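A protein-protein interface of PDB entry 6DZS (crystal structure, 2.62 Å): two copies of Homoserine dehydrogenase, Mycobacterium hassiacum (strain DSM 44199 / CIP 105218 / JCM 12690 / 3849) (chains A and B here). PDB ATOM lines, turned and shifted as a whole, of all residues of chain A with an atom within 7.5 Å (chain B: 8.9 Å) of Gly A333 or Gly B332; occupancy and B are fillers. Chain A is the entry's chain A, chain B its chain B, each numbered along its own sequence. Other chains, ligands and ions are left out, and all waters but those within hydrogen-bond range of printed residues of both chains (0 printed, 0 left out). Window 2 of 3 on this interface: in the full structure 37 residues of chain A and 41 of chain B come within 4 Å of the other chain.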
ATOM      1  N   HIS A 126     -25.819  11.032 -29.115  1.00  0.00           N
ATOM      2  CA  HIS A 126     -24.747  10.420 -28.331  1.00  0.00           C
ATOM      3  C   HIS A 126     -25.242  10.079 -26.923  1.00  0.00           C
ATOM      4  O   HIS A 126     -24.749  10.584 -25.913  1.00  0.00           O
ATOM      5  CB  HIS A 126     -23.516  11.334 -28.294  1.00  0.00           C
ATOM      6  CG  HIS A 126     -22.963  11.656 -29.650  1.00  0.00           C
ATOM      7  ND1 HIS A 126     -22.236  10.750 -30.393  1.00  0.00           N
ATOM      8  CD2 HIS A 126     -23.036  12.782 -30.400  1.00  0.00           C
ATOM      9  CE1 HIS A 126     -21.883  11.304 -31.539  1.00  0.00           C
ATOM     10  NE2 HIS A 126     -22.356  12.536 -31.568  1.00  0.00           N
ATOM     11  N   ASP A 128     -27.898   6.845 -24.663  1.00  0.00           N
ATOM     12  CA  ASP A 128     -28.323   5.452 -24.623  1.00  0.00           C
ATOM     13  C   ASP A 128     -29.814   5.293 -24.914  1.00  0.00           C
ATOM     14  O   ASP A 128     -30.620   6.199 -24.694  1.00  0.00           O
ATOM     15  CB  ASP A 128     -28.029   4.836 -23.252  1.00  0.00           C
ATOM     16  CG  ASP A 128     -26.550   4.654 -22.995  1.00  0.00           C
ATOM     17  OD1 ASP A 128     -25.830   4.235 -23.924  1.00  0.00           O
ATOM     18  OD2 ASP A 128     -26.108   4.929 -21.860  1.00  0.00           O
ATOM     19  N   TYR A 130     -32.184   1.951 -23.966  1.00  0.00           N
ATOM     20  CA  TYR A 130     -32.283   0.599 -23.432  1.00  0.00           C
ATOM     21  C   TYR A 130     -33.742   0.169 -23.338  1.00  0.00           C
ATOM     22  O   TYR A 130     -34.602   0.944 -22.906  1.00  0.00           O
ATOM     23  CB  TYR A 130     -31.624   0.518 -22.052  1.00  0.00           C
ATOM     24  CG  TYR A 130     -30.117   0.668 -22.063  1.00  0.00           C
ATOM     25  CD1 TYR A 130     -29.360   0.230 -23.143  1.00  0.00           C
ATOM     26  CD2 TYR A 130     -29.449   1.236 -20.987  1.00  0.00           C
ATOM     27  CE1 TYR A 130     -27.983   0.356 -23.154  1.00  0.00           C
ATOM     28  CE2 TYR A 130     -28.067   1.365 -20.989  1.00  0.00           C
ATOM     29  CZ  TYR A 130     -27.341   0.922 -22.076  1.00  0.00           C
ATOM     30  OH  TYR A 130     -25.971   1.047 -22.090  1.00  0.00           O
ATOM     31  N   MET A 324     -27.334   1.133 -15.645  1.00  0.00           N
ATOM     32  CA  MET A 324     -26.342   1.142 -16.713  1.00  0.00           C
ATOM     33  C   MET A 324     -26.308   2.494 -17.412  1.00  0.00           C
ATOM     34  O   MET A 324     -25.228   3.042 -17.667  1.00  0.00           O
ATOM     35  CB  MET A 324     -26.634   0.019 -17.708  1.00  0.00           C
ATOM     36  CG  MET A 324     -26.307  -1.375 -17.172  1.00  0.00           C
ATOM     37  SD  MET A 324     -24.596  -1.526 -16.608  1.00  0.00           S
ATOM     38  CE  MET A 324     -23.715  -1.096 -18.111  1.00  0.00           C
ATOM     39  N   ALA A 325     -27.479   3.060 -17.713  1.00  0.00           N
ATOM     40  CA  ALA A 325     -27.520   4.356 -18.379  1.00  0.00           C
ATOM     41  C   ALA A 325     -26.890   5.435 -17.513  1.00  0.00           C
ATOM     42  O   ALA A 325     -26.189   6.321 -18.021  1.00  0.00           O
ATOM     43  CB  ALA A 325     -28.959   4.724 -18.723  1.00  0.00           C
ATOM     44  N   ARG A 327     -24.563   4.872 -15.135  1.00  0.00           N
ATOM     45  CA  ARG A 327     -23.134   4.578 -15.133  1.00  0.00           C
ATOM     46  C   ARG A 327     -22.458   5.139 -16.378  1.00  0.00           C
ATOM     47  O   ARG A 327     -21.383   5.746 -16.297  1.00  0.00           O
ATOM     48  CB  ARG A 327     -22.907   3.068 -15.046  1.00  0.00           C
ATOM     49  CG  ARG A 327     -23.007   2.480 -13.650  1.00  0.00           C
ATOM     50  CD  ARG A 327     -23.015   0.963 -13.726  1.00  0.00           C
ATOM     51  NE  ARG A 327     -22.836   0.328 -12.424  1.00  0.00           N
ATOM     52  CZ  ARG A 327     -23.022  -0.969 -12.196  1.00  0.00           C
ATOM     53  NH1 ARG A 327     -23.408  -1.771 -13.182  1.00  0.00           N
ATOM     54  NH2 ARG A 327     -22.832  -1.467 -10.982  1.00  0.00           N
ATOM     55  N   ASN A 328     -23.072   4.940 -17.547  1.00  0.00           N
ATOM     56  CA  ASN A 328     -22.469   5.418 -18.785  1.00  0.00           C
ATOM     57  C   ASN A 328     -22.334   6.935 -18.781  1.00  0.00           C
ATOM     58  O   ASN A 328     -21.342   7.478 -19.281  1.00  0.00           O
ATOM     59  CB  ASN A 328     -23.289   4.954 -19.987  1.00  0.00           C
ATOM     60  CG  ASN A 328     -23.287   3.446 -20.145  1.00  0.00           C
ATOM     61  OD1 ASN A 328     -22.397   2.759 -19.646  1.00  0.00           O
ATOM     62  ND2 ASN A 328     -24.286   2.922 -20.846  1.00  0.00           N
ATOM     63  N   ARG A 329     -23.319   7.640 -18.223  1.00  0.00           N
ATOM     64  CA  ARG A 329     -23.231   9.095 -18.168  1.00  0.00           C
ATOM     65  C   ARG A 329     -22.167   9.543 -17.175  1.00  0.00           C
ATOM     66  O   ARG A 329     -21.478  10.543 -17.407  1.00  0.00           O
ATOM     67  CB  ARG A 329     -24.594   9.690 -17.820  1.00  0.00           C
ATOM     68  CG  ARG A 329     -25.615   9.527 -18.934  1.00  0.00           C
ATOM     69  CD  ARG A 329     -26.923  10.209 -18.604  1.00  0.00           C
ATOM     70  NE  ARG A 329     -26.829  11.663 -18.711  1.00  0.00           N
ATOM     71  CZ  ARG A 329     -27.062  12.353 -19.824  1.00  0.00           C
ATOM     72  NH1 ARG A 329     -27.397  11.731 -20.948  1.00  0.00           N
ATOM     73  NH2 ARG A 329     -26.958  13.675 -19.808  1.00  0.00           N
ATOM     74  N   VAL A 330     -22.004   8.812 -16.070  1.00  0.00           N
ATOM     75  CA  VAL A 330     -20.977   9.166 -15.096  1.00  0.00           C
ATOM     76  C   VAL A 330     -19.590   9.011 -15.707  1.00  0.00           C
ATOM     77  O   VAL A 330     -18.780   9.944 -15.696  1.00  0.00           O
ATOM     78  CB  VAL A 330     -21.129   8.314 -13.823  1.00  0.00           C
ATOM     79  CG1 VAL A 330     -19.917   8.478 -12.915  1.00  0.00           C
ATOM     80  CG2 VAL A 330     -22.396   8.698 -13.077  1.00  0.00           C
ATOM     81  N   GLN A 331     -19.296   7.831 -16.252  1.00  0.00           N
ATOM     82  CA  GLN A 331     -17.982   7.551 -16.814  1.00  0.00           C
ATOM     83  C   GLN A 331     -17.823   8.034 -18.248  1.00  0.00           C
ATOM     84  O   GLN A 331     -16.725   7.910 -18.803  1.00  0.00           O
ATOM     85  CB  GLN A 331     -17.700   6.048 -16.767  1.00  0.00           C
ATOM     86  CG  GLN A 331     -17.597   5.463 -15.375  1.00  0.00           C
ATOM     87  CD  GLN A 331     -17.278   3.977 -15.401  1.00  0.00           C
ATOM     88  OE1 GLN A 331     -16.395   3.531 -16.137  1.00  0.00           O
ATOM     89  NE2 GLN A 331     -18.005   3.200 -14.606  1.00  0.00           N
ATOM     90  N   GLY A 332     -18.869   8.572 -18.865  1.00  0.00           N
ATOM     91  CA  GLY A 332     -18.800   8.904 -20.274  1.00  0.00           C
ATOM     92  C   GLY A 332     -18.738   7.656 -21.131  1.00  0.00           C
ATOM     93  O   GLY A 332     -18.475   6.560 -20.623  1.00  0.00           O
ATOM     94  N   GLY A 333     -18.971   7.802 -22.431  1.00  0.00           N
ATOM     95  CA  GLY A 333     -19.046   6.650 -23.308  1.00  0.00           C
ATOM     96  C   GLY A 333     -20.373   5.931 -23.182  1.00  0.00           C
ATOM     97  O   GLY A 333     -20.850   5.683 -22.070  1.00  0.00           O
ATOM     98  N   ARG A 334     -20.978   5.590 -24.316  1.00  0.00           N
ATOM     99  CA  ARG A 334     -22.299   4.980 -24.329  1.00  0.00           C
ATOM    100  C   ARG A 334     -22.189   3.477 -24.081  1.00  0.00           C
ATOM    101  O   ARG A 334     -21.136   2.954 -23.707  1.00  0.00           O
ATOM    102  CB  ARG A 334     -23.001   5.259 -25.655  1.00  0.00           C
ATOM    103  CG  ARG A 334     -23.249   6.721 -25.944  1.00  0.00           C
ATOM    104  CD  ARG A 334     -23.992   6.890 -27.258  1.00  0.00           C
ATOM    105  NE  ARG A 334     -23.206   6.447 -28.406  1.00  0.00           N
ATOM    106  CZ  ARG A 334     -22.299   7.195 -29.031  1.00  0.00           C
ATOM    107  NH1 ARG A 334     -22.048   8.432 -28.621  1.00  0.00           N
ATOM    108  NH2 ARG A 334     -21.639   6.702 -30.069  1.00  0.00           N
ATOM    109  N   GLY A 335     -23.295   2.768 -24.292  1.00  0.00           N
ATOM    110  CA  GLY A 335     -23.312   1.328 -24.233  1.00  0.00           C
ATOM    111  C   GLY A 335     -23.220   0.751 -25.628  1.00  0.00           C
ATOM    112  O   GLY A 335     -22.562   1.316 -26.508  1.00  0.00           O
ATOM    113  N   HIS B 126      -7.613   3.161 -17.603  1.00  0.00           N
ATOM    114  CA  HIS B 126      -8.819   3.356 -18.403  1.00  0.00           C
ATOM    115  C   HIS B 126      -8.957   2.220 -19.405  1.00  0.00           C
ATOM    116  O   HIS B 126      -8.819   2.429 -20.614  1.00  0.00           O
ATOM    117  CB  HIS B 126      -8.789   4.711 -19.114  1.00  0.00           C
ATOM    118  CG  HIS B 126      -8.920   5.879 -18.185  1.00  0.00           C
ATOM    119  ND1 HIS B 126     -10.135   6.307 -17.695  1.00  0.00           N
ATOM    120  CD2 HIS B 126      -7.988   6.705 -17.652  1.00  0.00           C
ATOM    121  CE1 HIS B 126      -9.946   7.346 -16.902  1.00  0.00           C
ATOM    122  NE2 HIS B 126      -8.653   7.609 -16.858  1.00  0.00           N
ATOM    123  N   ASP B 128     -10.531  -2.196 -19.916  1.00  0.00           N
ATOM    124  CA  ASP B 128     -11.466  -3.226 -19.488  1.00  0.00           C
ATOM    125  C   ASP B 128     -10.739  -4.424 -18.890  1.00  0.00           C
ATOM    126  O   ASP B 128      -9.583  -4.707 -19.217  1.00  0.00           O
ATOM    127  CB  ASP B 128     -12.326  -3.710 -20.659  1.00  0.00           C
ATOM    128  CG  ASP B 128     -13.157  -2.610 -21.270  1.00  0.00           C
ATOM    129  OD1 ASP B 128     -13.932  -1.964 -20.533  1.00  0.00           O
ATOM    130  OD2 ASP B 128     -13.026  -2.394 -22.494  1.00  0.00           O
ATOM    131  N   MET B 324     -17.017  -7.190 -26.745  1.00  0.00           N
ATOM    132  CA  MET B 324     -17.338  -6.017 -25.941  1.00  0.00           C
ATOM    133  C   MET B 324     -16.097  -5.167 -25.694  1.00  0.00           C
ATOM    134  O   MET B 324     -16.151  -3.936 -25.815  1.00  0.00           O
ATOM    135  CB  MET B 324     -17.991  -6.449 -24.625  1.00  0.00           C
ATOM    136  CG  MET B 324     -19.401  -7.029 -24.800  1.00  0.00           C
ATOM    137  SD  MET B 324     -20.551  -5.894 -25.618  1.00  0.00           S
ATOM    138  CE  MET B 324     -20.614  -4.571 -24.414  1.00  0.00           C
ATOM    139  N   ALA B 325     -14.964  -5.799 -25.374  1.00  0.00           N
ATOM    140  CA  ALA B 325     -13.728  -5.046 -25.174  1.00  0.00           C
ATOM    141  C   ALA B 325     -13.278  -4.358 -26.457  1.00  0.00           C
ATOM    142  O   ALA B 325     -12.713  -3.258 -26.408  1.00  0.00           O
ATOM    143  CB  ALA B 325     -12.624  -5.968 -24.654  1.00  0.00           C
ATOM    144  N   ALA B 326     -13.512  -4.989 -27.610  1.00  0.00           N
ATOM    145  CA  ALA B 326     -13.169  -4.355 -28.877  1.00  0.00           C
ATOM    146  C   ALA B 326     -14.142  -3.232 -29.205  1.00  0.00           C
ATOM    147  O   ALA B 326     -13.727  -2.158 -29.657  1.00  0.00           O
ATOM    148  CB  ALA B 326     -13.151  -5.393 -29.998  1.00  0.00           C
ATOM    149  N   ARG B 327     -15.440  -3.460 -28.988  1.00  0.00           N
ATOM    150  CA  ARG B 327     -16.419  -2.389 -29.154  1.00  0.00           C
ATOM    151  C   ARG B 327     -16.048  -1.182 -28.301  1.00  0.00           C
ATOM    152  O   ARG B 327     -16.016  -0.047 -28.789  1.00  0.00           O
ATOM    153  CB  ARG B 327     -17.818  -2.884 -28.783  1.00  0.00           C
ATOM    154  CG  ARG B 327     -18.593  -3.567 -29.902  1.00  0.00           C
ATOM    155  CD  ARG B 327     -19.884  -4.168 -29.353  1.00  0.00           C
ATOM    156  NE  ARG B 327     -20.747  -4.713 -30.399  1.00  0.00           N
ATOM    157  CZ  ARG B 327     -21.760  -5.544 -30.171  1.00  0.00           C
ATOM    158  NH1 ARG B 327     -22.031  -5.941 -28.934  1.00  0.00           N
ATOM    159  NH2 ARG B 327     -22.496  -5.988 -31.182  1.00  0.00           N
ATOM    160  N   ASN B 328     -15.761  -1.413 -27.015  1.00  0.00           N
ATOM    161  CA  ASN B 328     -15.424  -0.310 -26.120  1.00  0.00           C
ATOM    162  C   ASN B 328     -14.223   0.475 -26.642  1.00  0.00           C
ATOM    163  O   ASN B 328     -14.244   1.711 -26.671  1.00  0.00           O
ATOM    164  CB  ASN B 328     -15.153  -0.835 -24.706  1.00  0.00           C
ATOM    165  CG  ASN B 328     -16.420  -1.264 -23.976  1.00  0.00           C
ATOM    166  OD1 ASN B 328     -16.480  -2.352 -23.407  1.00  0.00           O
ATOM    167  ND2 ASN B 328     -17.432  -0.404 -23.980  1.00  0.00           N
ATOM    168  N   ARG B 329     -13.163  -0.223 -27.066  1.00  0.00           N
ATOM    169  CA  ARG B 329     -11.979   0.482 -27.551  1.00  0.00           C
ATOM    170  C   ARG B 329     -12.262   1.245 -28.839  1.00  0.00           C
ATOM    171  O   ARG B 329     -11.600   2.250 -29.117  1.00  0.00           O
ATOM    172  CB  ARG B 329     -10.824  -0.490 -27.774  1.00  0.00           C
ATOM    173  CG  ARG B 329     -10.248  -1.059 -26.499  1.00  0.00           C
ATOM    174  CD  ARG B 329      -8.991  -1.854 -26.784  1.00  0.00           C
ATOM    175  NE  ARG B 329      -7.816  -1.003 -26.967  1.00  0.00           N
ATOM    176  CZ  ARG B 329      -6.978  -0.660 -25.992  1.00  0.00           C
ATOM    177  NH1 ARG B 329      -7.174  -1.080 -24.750  1.00  0.00           N
ATOM    178  NH2 ARG B 329      -5.935   0.108 -26.263  1.00  0.00           N
ATOM    179  N   VAL B 330     -13.223   0.785 -29.642  1.00  0.00           N
ATOM    180  CA  VAL B 330     -13.604   1.539 -30.831  1.00  0.00           C
ATOM    181  C   VAL B 330     -14.417   2.769 -30.442  1.00  0.00           C
ATOM    182  O   VAL B 330     -14.176   3.872 -30.949  1.00  0.00           O
ATOM    183  CB  VAL B 330     -14.377   0.636 -31.811  1.00  0.00           C
ATOM    184  CG1 VAL B 330     -15.023   1.464 -32.915  1.00  0.00           C
ATOM    185  CG2 VAL B 330     -13.450  -0.414 -32.410  1.00  0.00           C
ATOM    186  N   GLN B 331     -15.377   2.608 -29.530  1.00  0.00           N
ATOM    187  CA  GLN B 331     -16.330   3.659 -29.193  1.00  0.00           C
ATOM    188  C   GLN B 331     -15.934   4.477 -27.964  1.00  0.00           C
ATOM    189  O   GLN B 331     -16.742   5.279 -27.486  1.00  0.00           O
ATOM    190  CB  GLN B 331     -17.721   3.057 -28.964  1.00  0.00           C
ATOM    191  CG  GLN B 331     -18.313   2.318 -30.156  1.00  0.00           C
ATOM    192  CD  GLN B 331     -19.648   1.670 -29.826  1.00  0.00           C
ATOM    193  OE1 GLN B 331     -20.166   1.821 -28.717  1.00  0.00           O
ATOM    194  NE2 GLN B 331     -20.209   0.944 -30.785  1.00  0.00           N
ATOM    195  N   GLY B 332     -14.727   4.290 -27.434  1.00  0.00           N
ATOM    196  CA  GLY B 332     -14.255   5.111 -26.333  1.00  0.00           C
ATOM    197  C   GLY B 332     -15.082   5.006 -25.066  1.00  0.00           C
ATOM    198  O   GLY B 332     -15.734   5.973 -24.658  1.00  0.00           O
ATOM    199  N   GLY B 333     -15.051   3.842 -24.427  1.00  0.00           N
ATOM    200  CA  GLY B 333     -15.779   3.631 -23.198  1.00  0.00           C
ATOM    201  C   GLY B 333     -15.150   2.526 -22.379  1.00  0.00           C
ATOM    202  O   GLY B 333     -14.026   2.092 -22.643  1.00  0.00           O
ATOM    203  N   ARG B 334     -15.892   2.074 -21.373  1.00  0.00           N
ATOM    204  CA  ARG B 334     -15.435   1.006 -20.494  1.00  0.00           C
ATOM    205  C   ARG B 334     -16.651   0.202 -20.040  1.00  0.00           C
ATOM    206  O   ARG B 334     -17.770   0.413 -20.516  1.00  0.00           O
ATOM    207  CB  ARG B 334     -14.642   1.578 -19.310  1.00  0.00           C
ATOM    208  CG  ARG B 334     -13.204   1.953 -19.645  1.00  0.00           C
ATOM    209  CD  ARG B 334     -12.436   2.393 -18.404  1.00  0.00           C
ATOM    210  NE  ARG B 334     -12.878   3.696 -17.910  1.00  0.00           N
ATOM    211  CZ  ARG B 334     -12.410   4.285 -16.811  1.00  0.00           C
ATOM    212  NH1 ARG B 334     -11.480   3.691 -16.073  1.00  0.00           N
ATOM    213  NH2 ARG B 334     -12.876   5.473 -16.449  1.00  0.00           N
ATOM    214  N   GLY B 335     -16.423  -0.732 -19.119  1.00  0.00           N
ATOM    215  CA  GLY B 335     -17.486  -1.525 -18.551  1.00  0.00           C
ATOM    216  C   GLY B 335     -17.795  -1.103 -17.131  1.00  0.00           C
ATOM    217  O   GLY B 335     -17.196  -0.165 -16.593  1.00  0.00           O
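Gln A331 touches Arg B334, but with the chains exchanged Arg A334 does not touch Gln B331 (5.2 Å).
Gln A331 touches Gly B335, and with the chains exchanged Gly A335 touches Gln B331.
Gly A333 touches Gly B332, but with the chains exchanged Gly A332 does not touch Gly B333 (4.7 Å).
13 positions are printed for both chains.
Gly A333 touches just one residue of chain B: Gly B332.
Gly B332 touches one residue of chain A.
No residue of chain B comes within 4 Å of Gly A332.
Of the printed residues of chain A, Gln B331 touches Gly A335 (3.3 Å).
Printed residues of chain A within 4 Å of Gly B335: Gln A331.
Printed residues of chain B within 4 Å of Gly A335: Gln B331.
Printed residues of chain B within 4 Å of Gln A331: Arg B334 (3.9 Å) and Gly B335 (3.8 Å).
The nearest residue of chain A that does not touch Gly B332 is Gly A332 (4.9 Å).
The side-chain carboxylate of Asp B128 is in hydrogen-bond range of the backbone NH of Gly B335.
OD1 of Asp A128 lies within hydrogen-bond range of N of Gly A335, 3.0 Å away.
NH2 of Arg B334 lies within hydrogen-bond range of ND1 of His B126, 3.1 Å away.
Among the printed residues, pairs that only touch across the chains: Gly A333 with Gly B332 (3.6 Å), Gln A331 with Gly B335 (3.8 Å) and Gln A331 with Arg B334 (3.9 Å).
O of Gly A335 lies close to OE1 of Gln B331, 3.3 Å away.
Printed residues of chain A that touch a printed residue of chain B: Gln A331, Gly A333 and Gly A335.
Along chain A the printed residues that touch a printed residue of chain B span positions 331 to 335.
Of the 14 printed residues of chain B, 4 touch a printed residue of chain A.
Printed residues of chain B that touch a printed residue of chain A: Gln B331, Gly B332, Arg B334 and Gly B335.
Among the printed residues, no Asp or Glu carboxylate lies within 4 Å of a Lys or Arg side-chain nitrogen of the other chain.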
